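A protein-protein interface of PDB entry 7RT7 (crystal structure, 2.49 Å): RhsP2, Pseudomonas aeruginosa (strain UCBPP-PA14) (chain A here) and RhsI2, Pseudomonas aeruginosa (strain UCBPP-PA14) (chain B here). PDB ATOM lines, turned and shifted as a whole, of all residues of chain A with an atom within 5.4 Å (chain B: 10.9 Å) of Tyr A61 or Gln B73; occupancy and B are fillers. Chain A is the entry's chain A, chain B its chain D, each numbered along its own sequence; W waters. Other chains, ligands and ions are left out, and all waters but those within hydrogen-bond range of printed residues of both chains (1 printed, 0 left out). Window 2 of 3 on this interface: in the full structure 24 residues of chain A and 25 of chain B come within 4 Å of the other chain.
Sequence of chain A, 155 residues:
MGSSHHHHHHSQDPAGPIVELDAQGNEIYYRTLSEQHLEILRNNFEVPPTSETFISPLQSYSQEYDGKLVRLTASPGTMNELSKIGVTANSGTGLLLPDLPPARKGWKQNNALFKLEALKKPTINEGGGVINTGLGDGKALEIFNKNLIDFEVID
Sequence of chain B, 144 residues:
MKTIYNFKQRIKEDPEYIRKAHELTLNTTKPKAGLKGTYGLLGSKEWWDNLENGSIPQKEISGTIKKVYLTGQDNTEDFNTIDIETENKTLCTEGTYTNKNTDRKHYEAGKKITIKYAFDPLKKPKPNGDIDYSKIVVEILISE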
ATOM      1  N   TYR A  30      17.414   8.643 -21.093  1.00  0.00           N
ATOM      2  CA  TYR A  30      17.223   7.204 -21.164  1.00  0.00           C
ATOM      3  C   TYR A  30      18.553   6.522 -21.431  1.00  0.00           C
ATOM      4  O   TYR A  30      19.434   7.077 -22.093  1.00  0.00           O
ATOM      5  CB  TYR A  30      16.218   6.829 -22.255  1.00  0.00           C
ATOM      6  CG  TYR A  30      14.844   7.402 -22.020  1.00  0.00           C
ATOM      7  CD1 TYR A  30      13.932   6.745 -21.207  1.00  0.00           C
ATOM      8  CD2 TYR A  30      14.464   8.603 -22.599  1.00  0.00           C
ATOM      9  CE1 TYR A  30      12.675   7.266 -20.983  1.00  0.00           C
ATOM     10  CE2 TYR A  30      13.209   9.132 -22.381  1.00  0.00           C
ATOM     11  CZ  TYR A  30      12.319   8.460 -21.572  1.00  0.00           C
ATOM     12  OH  TYR A  30      11.065   8.982 -21.351  1.00  0.00           O
ATOM     13  N   ARG A  31      18.683   5.305 -20.911  1.00  0.00           N
ATOM     14  CA  ARG A  31      19.861   4.488 -21.152  1.00  0.00           C
ATOM     15  C   ARG A  31      19.542   3.049 -20.778  1.00  0.00           C
ATOM     16  O   ARG A  31      18.870   2.800 -19.773  1.00  0.00           O
ATOM     17  CB  ARG A  31      21.059   5.005 -20.349  1.00  0.00           C
ATOM     18  CG  ARG A  31      22.380   4.342 -20.691  1.00  0.00           C
ATOM     19  CD  ARG A  31      23.503   4.934 -19.842  1.00  0.00           C
ATOM     20  NE  ARG A  31      24.617   4.010 -19.668  1.00  0.00           N
ATOM     21  CZ  ARG A  31      25.472   3.680 -20.629  1.00  0.00           C
ATOM     22  NH1 ARG A  31      25.323   4.116 -21.868  1.00  0.00           N
ATOM     23  NH2 ARG A  31      26.497   2.887 -20.336  1.00  0.00           N
ATOM     24  N   THR A  32      20.018   2.110 -21.592  1.00  0.00           N
ATOM     25  CA  THR A  32      19.881   0.682 -21.324  1.00  0.00           C
ATOM     26  C   THR A  32      21.204   0.161 -20.776  1.00  0.00           C
ATOM     27  O   THR A  32      22.251   0.337 -21.408  1.00  0.00           O
ATOM     28  CB  THR A  32      19.490  -0.084 -22.589  1.00  0.00           C
ATOM     29  OG1 THR A  32      18.274   0.453 -23.124  1.00  0.00           O
ATOM     30  CG2 THR A  32      19.294  -1.561 -22.282  1.00  0.00           C
ATOM     31  N   LEU A  33      21.156  -0.472 -19.604  1.00  0.00           N
ATOM     32  CA  LEU A  33      22.356  -0.779 -18.840  1.00  0.00           C
ATOM     33  C   LEU A  33      22.494  -2.271 -18.579  1.00  0.00           C
ATOM     34  O   LEU A  33      21.536  -3.044 -18.680  1.00  0.00           O
ATOM     35  CB  LEU A  33      22.361  -0.041 -17.489  1.00  0.00           C
ATOM     36  CG  LEU A  33      22.958   1.364 -17.511  1.00  0.00           C
ATOM     37  CD1 LEU A  33      22.096   2.231 -18.375  1.00  0.00           C
ATOM     38  CD2 LEU A  33      23.065   1.996 -16.136  1.00  0.00           C
ATOM     39  N   THR A  50      31.278   3.721 -19.252  1.00  0.00           N
ATOM     40  CA  THR A  50      31.685   2.727 -20.240  1.00  0.00           C
ATOM     41  C   THR A  50      31.727   3.374 -21.624  1.00  0.00           C
ATOM     42  O   THR A  50      30.684   3.724 -22.188  1.00  0.00           O
ATOM     43  CB  THR A  50      30.749   1.514 -20.232  1.00  0.00           C
ATOM     44  OG1 THR A  50      31.169   0.575 -21.231  1.00  0.00           O
ATOM     45  CG2 THR A  50      29.316   1.922 -20.502  1.00  0.00           C
ATOM     46  N   PHE A  54      26.494   6.966 -23.376  1.00  0.00           N
ATOM     47  CA  PHE A  54      25.483   7.756 -24.060  1.00  0.00           C
ATOM     48  C   PHE A  54      24.172   7.747 -23.285  1.00  0.00           C
ATOM     49  O   PHE A  54      23.725   6.706 -22.796  1.00  0.00           O
ATOM     50  CB  PHE A  54      25.238   7.220 -25.473  1.00  0.00           C
ATOM     51  CG  PHE A  54      26.166   7.784 -26.512  1.00  0.00           C
ATOM     52  CD1 PHE A  54      26.299   9.153 -26.680  1.00  0.00           C
ATOM     53  CD2 PHE A  54      26.896   6.942 -27.333  1.00  0.00           C
ATOM     54  CE1 PHE A  54      27.151   9.669 -27.637  1.00  0.00           C
ATOM     55  CE2 PHE A  54      27.748   7.452 -28.293  1.00  0.00           C
ATOM     56  CZ  PHE A  54      27.875   8.818 -28.445  1.00  0.00           C
ATOM     57  N   SER A  56      20.077   9.286 -23.873  1.00  0.00           N
ATOM     58  CA  SER A  56      19.222   9.652 -24.991  1.00  0.00           C
ATOM     59  C   SER A  56      18.011  10.437 -24.506  1.00  0.00           C
ATOM     60  O   SER A  56      17.450  10.128 -23.449  1.00  0.00           O
ATOM     61  CB  SER A  56      18.751   8.403 -25.753  1.00  0.00           C
ATOM     62  OG  SER A  56      18.096   8.761 -26.957  1.00  0.00           O
ATOM     63  N   LEU A  58      15.205  10.300 -25.969  1.00  0.00           N
ATOM     64  CA  LEU A  58      14.057   9.557 -26.467  1.00  0.00           C
ATOM     65  C   LEU A  58      14.140   8.116 -25.988  1.00  0.00           C
ATOM     66  O   LEU A  58      15.203   7.493 -26.059  1.00  0.00           O
ATOM     67  CB  LEU A  58      13.996   9.600 -27.998  1.00  0.00           C
ATOM     68  CG  LEU A  58      13.541  10.923 -28.618  1.00  0.00           C
ATOM     69  CD1 LEU A  58      13.595  10.848 -30.136  1.00  0.00           C
ATOM     70  CD2 LEU A  58      12.141  11.280 -28.156  1.00  0.00           C
ATOM     71  N   GLN A  59      13.013   7.595 -25.499  1.00  0.00           N
ATOM     72  CA  GLN A  59      12.966   6.202 -25.072  1.00  0.00           C
ATOM     73  C   GLN A  59      13.095   5.256 -26.261  1.00  0.00           C
ATOM     74  O   GLN A  59      13.700   4.184 -26.145  1.00  0.00           O
ATOM     75  CB  GLN A  59      11.664   5.933 -24.318  1.00  0.00           C
ATOM     76  CG  GLN A  59      11.518   4.509 -23.809  1.00  0.00           C
ATOM     77  CD  GLN A  59      10.208   4.285 -23.080  1.00  0.00           C
ATOM     78  OE1 GLN A  59       9.727   5.162 -22.360  1.00  0.00           O
ATOM     79  NE2 GLN A  59       9.620   3.109 -23.266  1.00  0.00           N
ATOM     80  N   SER A  60      12.529   5.637 -27.410  1.00  0.00           N
ATOM     81  CA  SER A  60      12.533   4.749 -28.568  1.00  0.00           C
ATOM     82  C   SER A  60      13.942   4.337 -28.961  1.00  0.00           C
ATOM     83  O   SER A  60      14.133   3.266 -29.548  1.00  0.00           O
ATOM     84  CB  SER A  60      11.843   5.423 -29.754  1.00  0.00           C
ATOM     85  OG  SER A  60      12.274   6.763 -29.885  1.00  0.00           O
ATOM     86  N   TYR A  61      14.943   5.169 -28.665  1.00  0.00           N
ATOM     87  CA  TYR A  61      16.312   4.809 -29.014  1.00  0.00           C
ATOM     88  C   TYR A  61      16.843   3.720 -28.087  1.00  0.00           C
ATOM     89  O   TYR A  61      17.236   2.640 -28.538  1.00  0.00           O
ATOM     90  CB  TYR A  61      17.226   6.033 -28.964  1.00  0.00           C
ATOM     91  CG  TYR A  61      18.671   5.671 -29.229  1.00  0.00           C
ATOM     92  CD1 TYR A  61      19.146   5.544 -30.527  1.00  0.00           C
ATOM     93  CD2 TYR A  61      19.551   5.426 -28.182  1.00  0.00           C
ATOM     94  CE1 TYR A  61      20.460   5.200 -30.777  1.00  0.00           C
ATOM     95  CE2 TYR A  61      20.867   5.080 -28.422  1.00  0.00           C
ATOM     96  CZ  TYR A  61      21.316   4.969 -29.722  1.00  0.00           C
ATOM     97  OH  TYR A  61      22.624   4.627 -29.968  1.00  0.00           O
ATOM     98  N   SER A  62      16.863   3.992 -26.780  1.00  0.00           N
ATOM     99  CA  SER A  62      17.464   3.047 -25.844  1.00  0.00           C
ATOM    100  C   SER A  62      16.659   1.757 -25.742  1.00  0.00           C
ATOM    101  O   SER A  62      17.231   0.694 -25.469  1.00  0.00           O
ATOM    102  CB  SER A  62      17.603   3.688 -24.464  1.00  0.00           C
ATOM    103  OG  SER A  62      18.666   4.624 -24.449  1.00  0.00           O
ATOM    104  N   GLN A  63      15.344   1.824 -25.955  1.00  0.00           N
ATOM    105  CA  GLN A  63      14.520   0.620 -25.901  1.00  0.00           C
ATOM    106  C   GLN A  63      14.973  -0.415 -26.921  1.00  0.00           C
ATOM    107  O   GLN A  63      14.698  -1.608 -26.742  1.00  0.00           O
ATOM    108  CB  GLN A  63      13.047   1.002 -26.108  1.00  0.00           C
ATOM    109  CG  GLN A  63      12.137  -0.075 -26.700  1.00  0.00           C
ATOM    110  CD  GLN A  63      10.877   0.513 -27.314  1.00  0.00           C
ATOM    111  OE1 GLN A  63      10.763   1.729 -27.479  1.00  0.00           O
ATOM    112  NE2 GLN A  63       9.925  -0.347 -27.656  1.00  0.00           N
ATOM    113  N   GLU A  64      15.662   0.011 -27.979  1.00  0.00           N
ATOM    114  CA  GLU A  64      16.147  -0.902 -29.005  1.00  0.00           C
ATOM    115  C   GLU A  64      17.254  -1.824 -28.512  1.00  0.00           C
ATOM    116  O   GLU A  64      17.644  -2.738 -29.248  1.00  0.00           O
ATOM    117  CB  GLU A  64      16.653  -0.096 -30.206  1.00  0.00           C
ATOM    118  CG  GLU A  64      15.553   0.551 -31.028  1.00  0.00           C
ATOM    119  CD  GLU A  64      14.621  -0.467 -31.652  1.00  0.00           C
ATOM    120  OE1 GLU A  64      15.077  -1.595 -31.933  1.00  0.00           O
ATOM    121  OE2 GLU A  64      13.433  -0.139 -31.858  1.00  0.00           O
ATOM    122  N   TYR A  65      17.763  -1.619 -27.301  1.00  0.00           N
ATOM    123  CA  TYR A  65      18.889  -2.379 -26.781  1.00  0.00           C
ATOM    124  C   TYR A  65      18.429  -3.434 -25.782  1.00  0.00           C
ATOM    125  O   TYR A  65      17.363  -3.327 -25.168  1.00  0.00           O
ATOM    126  CB  TYR A  65      19.904  -1.450 -26.108  1.00  0.00           C
ATOM    127  CG  TYR A  65      20.666  -0.560 -27.062  1.00  0.00           C
ATOM    128  CD1 TYR A  65      20.074   0.566 -27.619  1.00  0.00           C
ATOM    129  CD2 TYR A  65      21.984  -0.841 -27.400  1.00  0.00           C
ATOM    130  CE1 TYR A  65      20.771   1.384 -28.488  1.00  0.00           C
ATOM    131  CE2 TYR A  65      22.690  -0.027 -28.267  1.00  0.00           C
ATOM    132  CZ  TYR A  65      22.078   1.083 -28.808  1.00  0.00           C
ATOM    133  OH  TYR A  65      22.777   1.894 -29.673  1.00  0.00           O
ATOM    134  N   GLU A 117      22.204  10.059 -34.353  1.00  0.00           N
ATOM    135  CA  GLU A 117      22.123   8.637 -34.648  1.00  0.00           C
ATOM    136  C   GLU A 117      20.694   8.247 -34.987  1.00  0.00           C
ATOM    137  O   GLU A 117      19.741   8.984 -34.721  1.00  0.00           O
ATOM    138  CB  GLU A 117      22.621   7.789 -33.470  1.00  0.00           C
ATOM    139  CG  GLU A 117      24.134   7.715 -33.369  1.00  0.00           C
ATOM    140  CD  GLU A 117      24.617   7.371 -31.971  1.00  0.00           C
ATOM    141  OE1 GLU A 117      24.029   7.877 -30.993  1.00  0.00           O
ATOM    142  OE2 GLU A 117      25.589   6.595 -31.851  1.00  0.00           O
ATOM    143  N   ALA A 118      20.564   7.066 -35.592  1.00  0.00           N
ATOM    144  CA  ALA A 118      19.270   6.437 -35.836  1.00  0.00           C
ATOM    145  C   ALA A 118      18.422   7.249 -36.812  1.00  0.00           C
ATOM    146  O   ALA A 118      17.208   7.370 -36.647  1.00  0.00           O
ATOM    147  CB  ALA A 118      18.513   6.211 -34.524  1.00  0.00           C
ATOM    148  N   ILE A 124      11.911   5.762 -34.290  1.00  0.00           N
ATOM    149  CA  ILE A 124      12.541   6.860 -33.567  1.00  0.00           C
ATOM    150  C   ILE A 124      12.309   8.142 -34.358  1.00  0.00           C
ATOM    151  O   ILE A 124      12.970   8.400 -35.370  1.00  0.00           O
ATOM    152  CB  ILE A 124      14.035   6.608 -33.331  1.00  0.00           C
ATOM    153  CG1 ILE A 124      14.277   5.151 -32.919  1.00  0.00           C
ATOM    154  CG2 ILE A 124      14.561   7.547 -32.253  1.00  0.00           C
ATOM    155  CD1 ILE A 124      15.737   4.764 -32.861  1.00  0.00           C
ATOM    156  N   VAL A 130      17.943  11.346 -33.804  1.00  0.00           N
ATOM    157  CA  VAL A 130      18.016  11.795 -32.420  1.00  0.00           C
ATOM    158  C   VAL A 130      19.457  12.152 -32.088  1.00  0.00           C
ATOM    159  O   VAL A 130      20.394  11.469 -32.514  1.00  0.00           O
ATOM    160  CB  VAL A 130      17.488  10.724 -31.443  1.00  0.00           C
ATOM    161  CG1 VAL A 130      18.432   9.529 -31.398  1.00  0.00           C
ATOM    162  CG2 VAL A 130      17.308  11.323 -30.059  1.00  0.00           C
ATOM    163  N   ASN A 132      21.973  12.126 -29.304  1.00  0.00           N
ATOM    164  CA  ASN A 132      22.304  11.572 -28.002  1.00  0.00           C
ATOM    165  C   ASN A 132      23.484  12.331 -27.402  1.00  0.00           C
ATOM    166  O   ASN A 132      24.186  13.082 -28.081  1.00  0.00           O
ATOM    167  CB  ASN A 132      22.619  10.082 -28.123  1.00  0.00           C
ATOM    168  CG  ASN A 132      21.417   9.271 -28.568  1.00  0.00           C
ATOM    169  OD1 ASN A 132      20.281   9.738 -28.504  1.00  0.00           O
ATOM    170  ND2 ASN A 132      21.664   8.050 -29.027  1.00  0.00           N
ATOM    171  N   TYR B  69      25.839 -13.547 -23.630  1.00  0.00           N
ATOM    172  CA  TYR B  69      25.613 -12.501 -24.616  1.00  0.00           C
ATOM    173  C   TYR B  69      25.908 -11.148 -23.980  1.00  0.00           C
ATOM    174  O   TYR B  69      26.498 -11.058 -22.898  1.00  0.00           O
ATOM    175  CB  TYR B  69      24.187 -12.594 -25.181  1.00  0.00           C
ATOM    176  CG  TYR B  69      23.069 -12.378 -24.178  1.00  0.00           C
ATOM    177  CD1 TYR B  69      22.914 -13.215 -23.079  1.00  0.00           C
ATOM    178  CD2 TYR B  69      22.153 -11.348 -24.348  1.00  0.00           C
ATOM    179  CE1 TYR B  69      21.886 -13.023 -22.173  1.00  0.00           C
ATOM    180  CE2 TYR B  69      21.124 -11.149 -23.447  1.00  0.00           C
ATOM    181  CZ  TYR B  69      20.995 -11.989 -22.363  1.00  0.00           C
ATOM    182  OH  TYR B  69      19.969 -11.793 -21.466  1.00  0.00           O
ATOM    183  N   LEU B  70      25.496 -10.086 -24.670  1.00  0.00           N
ATOM    184  CA  LEU B  70      25.855  -8.718 -24.324  1.00  0.00           C
ATOM    185  C   LEU B  70      24.594  -7.878 -24.203  1.00  0.00           C
ATOM    186  O   LEU B  70      23.762  -7.866 -25.117  1.00  0.00           O
ATOM    187  CB  LEU B  70      26.787  -8.122 -25.387  1.00  0.00           C
ATOM    188  CG  LEU B  70      27.806  -7.075 -24.942  1.00  0.00           C
ATOM    189  CD1 LEU B  70      29.010  -7.088 -25.870  1.00  0.00           C
ATOM    190  CD2 LEU B  70      27.183  -5.700 -24.914  1.00  0.00           C
ATOM    191  N   THR B  71      24.456  -7.186 -23.077  1.00  0.00           N
ATOM    192  CA  THR B  71      23.366  -6.253 -22.844  1.00  0.00           C
ATOM    193  C   THR B  71      23.946  -4.886 -22.500  1.00  0.00           C
ATOM    194  O   THR B  71      25.121  -4.762 -22.145  1.00  0.00           O
ATOM    195  CB  THR B  71      22.447  -6.734 -21.715  1.00  0.00           C
ATOM    196  OG1 THR B  71      23.202  -6.856 -20.502  1.00  0.00           O
ATOM    197  CG2 THR B  71      21.832  -8.083 -22.062  1.00  0.00           C
ATOM    198  N   GLY B  72      23.112  -3.857 -22.610  1.00  0.00           N
ATOM    199  CA  GLY B  72      23.546  -2.507 -22.319  1.00  0.00           C
ATOM    200  C   GLY B  72      24.165  -1.820 -23.517  1.00  0.00           C
ATOM    201  O   GLY B  72      24.360  -2.398 -24.591  1.00  0.00           O
ATOM    202  N   GLN B  73      24.485  -0.544 -23.320  1.00  0.00           N
ATOM    203  CA  GLN B  73      25.041   0.298 -24.367  1.00  0.00           C
ATOM    204  C   GLN B  73      26.519   0.577 -24.119  1.00  0.00           C
ATOM    205  O   GLN B  73      26.992   0.562 -22.979  1.00  0.00           O
ATOM    206  CB  GLN B  73      24.304   1.639 -24.458  1.00  0.00           C
ATOM    207  CG  GLN B  73      22.829   1.547 -24.799  1.00  0.00           C
ATOM    208  CD  GLN B  73      22.179   2.916 -24.934  1.00  0.00           C
ATOM    209  OE1 GLN B  73      21.051   3.124 -24.487  1.00  0.00           O
ATOM    210  NE2 GLN B  73      22.888   3.856 -25.554  1.00  0.00           N
ATOM    211  N   ASP B  74      27.238   0.842 -25.209  1.00  0.00           N
ATOM    212  CA  ASP B  74      28.602   1.368 -25.153  1.00  0.00           C
ATOM    213  C   ASP B  74      29.547   0.447 -24.390  1.00  0.00           C
ATOM    214  O   ASP B  74      30.466   0.909 -23.710  1.00  0.00           O
ATOM    215  CB  ASP B  74      28.621   2.767 -24.529  1.00  0.00           C
ATOM    216  CG  ASP B  74      27.482   3.637 -25.016  1.00  0.00           C
ATOM    217  OD1 ASP B  74      27.082   3.492 -26.190  1.00  0.00           O
ATOM    218  OD2 ASP B  74      26.986   4.467 -24.225  1.00  0.00           O
ATOM    219  N   ASN B  75      29.338  -0.861 -24.495  1.00  0.00           N
ATOM    220  CA  ASN B  75      30.179  -1.829 -23.808  1.00  0.00           C
ATOM    221  C   ASN B  75      31.378  -2.194 -24.672  1.00  0.00           C
ATOM    222  O   ASN B  75      31.263  -2.325 -25.895  1.00  0.00           O
ATOM    223  CB  ASN B  75      29.381  -3.088 -23.468  1.00  0.00           C
ATOM    224  CG  ASN B  75      28.287  -2.831 -22.447  1.00  0.00           C
ATOM    225  OD1 ASN B  75      27.169  -3.322 -22.589  1.00  0.00           O
ATOM    226  ND2 ASN B  75      28.606  -2.066 -21.409  1.00  0.00           N
ATOM    227  N   THR B  76      32.530  -2.365 -24.025  1.00  0.00           N
ATOM    228  CA  THR B  76      33.762  -2.703 -24.726  1.00  0.00           C
ATOM    229  C   THR B  76      33.998  -4.206 -24.799  1.00  0.00           C
ATOM    230  O   THR B  76      34.464  -4.711 -25.827  1.00  0.00           O
ATOM    231  CB  THR B  76      34.957  -2.038 -24.036  1.00  0.00           C
ATOM    232  OG1 THR B  76      34.562  -0.762 -23.516  1.00  0.00           O
ATOM    233  CG2 THR B  76      36.108  -1.855 -25.012  1.00  0.00           C
ATOM    234  N   GLU B  77      33.681  -4.932 -23.730  1.00  0.00           N
ATOM    235  CA  GLU B  77      34.037  -6.337 -23.622  1.00  0.00           C
ATOM    236  C   GLU B  77      33.064  -7.207 -24.420  1.00  0.00           C
ATOM    237  O   GLU B  77      32.111  -6.723 -25.037  1.00  0.00           O
ATOM    238  CB  GLU B  77      34.080  -6.751 -22.153  1.00  0.00           C
ATOM    239  CG  GLU B  77      35.175  -6.053 -21.355  1.00  0.00           C
ATOM    240  CD  GLU B  77      34.626  -5.049 -20.363  1.00  0.00           C
ATOM    241  OE1 GLU B  77      34.360  -3.897 -20.766  1.00  0.00           O
ATOM    242  OE2 GLU B  77      34.464  -5.411 -19.178  1.00  0.00           O
ATOM    243  N   ASN B  80      28.586  -9.638 -20.881  1.00  0.00           N
ATOM    244  CA  ASN B  80      28.363  -9.153 -19.526  1.00  0.00           C
ATOM    245  C   ASN B  80      27.114  -9.740 -18.882  1.00  0.00           C
ATOM    246  O   ASN B  80      26.778  -9.340 -17.763  1.00  0.00           O
ATOM    247  CB  ASN B  80      28.262  -7.615 -19.505  1.00  0.00           C
ATOM    248  CG  ASN B  80      27.196  -7.090 -20.444  1.00  0.00           C
ATOM    249  OD1 ASN B  80      26.291  -7.821 -20.845  1.00  0.00           O
ATOM    250  ND2 ASN B  80      27.294  -5.813 -20.794  1.00  0.00           N
ATOM    251  N   THR B  81      26.419 -10.670 -19.535  1.00  0.00           N
ATOM    252  CA  THR B  81      25.148 -11.172 -19.026  1.00  0.00           C
ATOM    253  C   THR B  81      24.974 -12.626 -19.432  1.00  0.00           C
ATOM    254  O   THR B  81      25.475 -13.059 -20.472  1.00  0.00           O
ATOM    255  CB  THR B  81      23.967 -10.340 -19.549  1.00  0.00           C
ATOM    256  OG1 THR B  81      24.112  -8.986 -19.109  1.00  0.00           O
ATOM    257  CG2 THR B  81      22.637 -10.891 -19.055  1.00  0.00           C
HETATM  258  O   HOH W   1      33.845  -0.784 -20.976  1.00  0.00           O
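Of chain B, only Gln B73 (3.6 Å) and Asp B74 (2.9 Å) come within 4 Å of Arg A31. Of the printed residues of chain B, Leu A33 touches Gly B72. Thr A50 touches three residues of chain B. No residue of chain B comes within 4 Å of Leu A58. No residue of chain B comes within 4 Å of Ser A60. Tyr A61 touches one residue of chain B. Printed residues of chain B within 4 Å of Ser A62: Gln B73. Printed residues of chain B within 4 Å of Tyr A65: Gly B72 (3.995 Å) and Gln B73 (3.6 Å). Glu A117 touches none of the printed residues of chain B. No residue of chain B comes within 4 Å of Ala A118. No residue of chain B comes within 4 Å of Val A130. Gln B73 touches just these residues of chain A: Arg A31 (3.6 Å), Thr A32 (3.1 Å), Thr A50 (3.7 Å), Tyr A61 (3.7 Å), Ser A62 (2.8 Å) and Tyr A65 (3.6 Å). Of the printed residues of chain A, Asp B74 touches Arg A31 (2.9 Å), Thr A50 (2.6 Å) and Phe A54 (2.7 Å). Of the printed residues of chain A, Asn B75 touches Thr A50 (3.7 Å). The nearest residue of chain B that does not touch Tyr A61 is Asp B74 (6.0 Å). The nearest printed residue of chain A that does not touch Asp B74 is Tyr A65 (5.5 Å).
NH1 of Arg A31 is in salt-bridge range of OD2 of Asp B74, at 2.9 Å. The backbone NH (N) of Gln B73 lies within hydrogen-bond range of the backbone carbonyl oxygen (O) of Thr A32, at 3.1 Å. OG1 of Thr A50 sits at hydrogen-bond distance from O of Asp B74 (2.6 Å). The backbone NH of Phe A54 lies within hydrogen-bond range of the side-chain carboxylate of Asp B74 (2.7 Å). The side-chain amide oxygen (OE1) of Gln B73 lies within hydrogen-bond range of the side-chain hydroxyl (OG) of Ser A62.
NH2 of Arg A31 touches O of Gln B73, 3.6 Å away. Thr A32 touches Gly B72 (O to CA, 3.3 Å). Gly B72 touches Leu A33 (CA to C, 3.9 Å). CG2 of Thr A50 touches O of Gln B73, at 3.7 Å. Thr A50 touches Asn B75. Tyr A61 touches Gln B73. CD2 of Tyr A65 touches O of Gly B72 (3.995 Å). CG of Gln B73 touches CD2 of Tyr A65, 3.6 Å away.
Water W1 lies within hydrogen-bond range of the side-chain hydroxyl (OG1) of Thr B76 (2.6 Å), the side-chain hydroxyl (OG1) of Thr A50 (3.0 Å) and the side-chain carboxylate (OE1) of Glu B77 (3.2 Å).
O of Tyr A30 sits at hydrogen-bond distance from OG of Ser A62. The side-chain hydroxyl of Thr A32 is in hydrogen-bond range of the backbone carbonyl oxygen of Ser A62 (2.6 Å). OH of Tyr A61 sits at hydrogen-bond distance from OH of Tyr A65, at 2.8 Å. The backbone carbonyl oxygen of Thr B71 lies close to the side-chain amide oxygen of Asn B75 (2.5 Å). ND2 of Asn B75 sits at hydrogen-bond distance from O of Gln B73. OD1 of Asn B75 sits at hydrogen-bond distance from ND2 of Asn B80 (3.1 Å).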
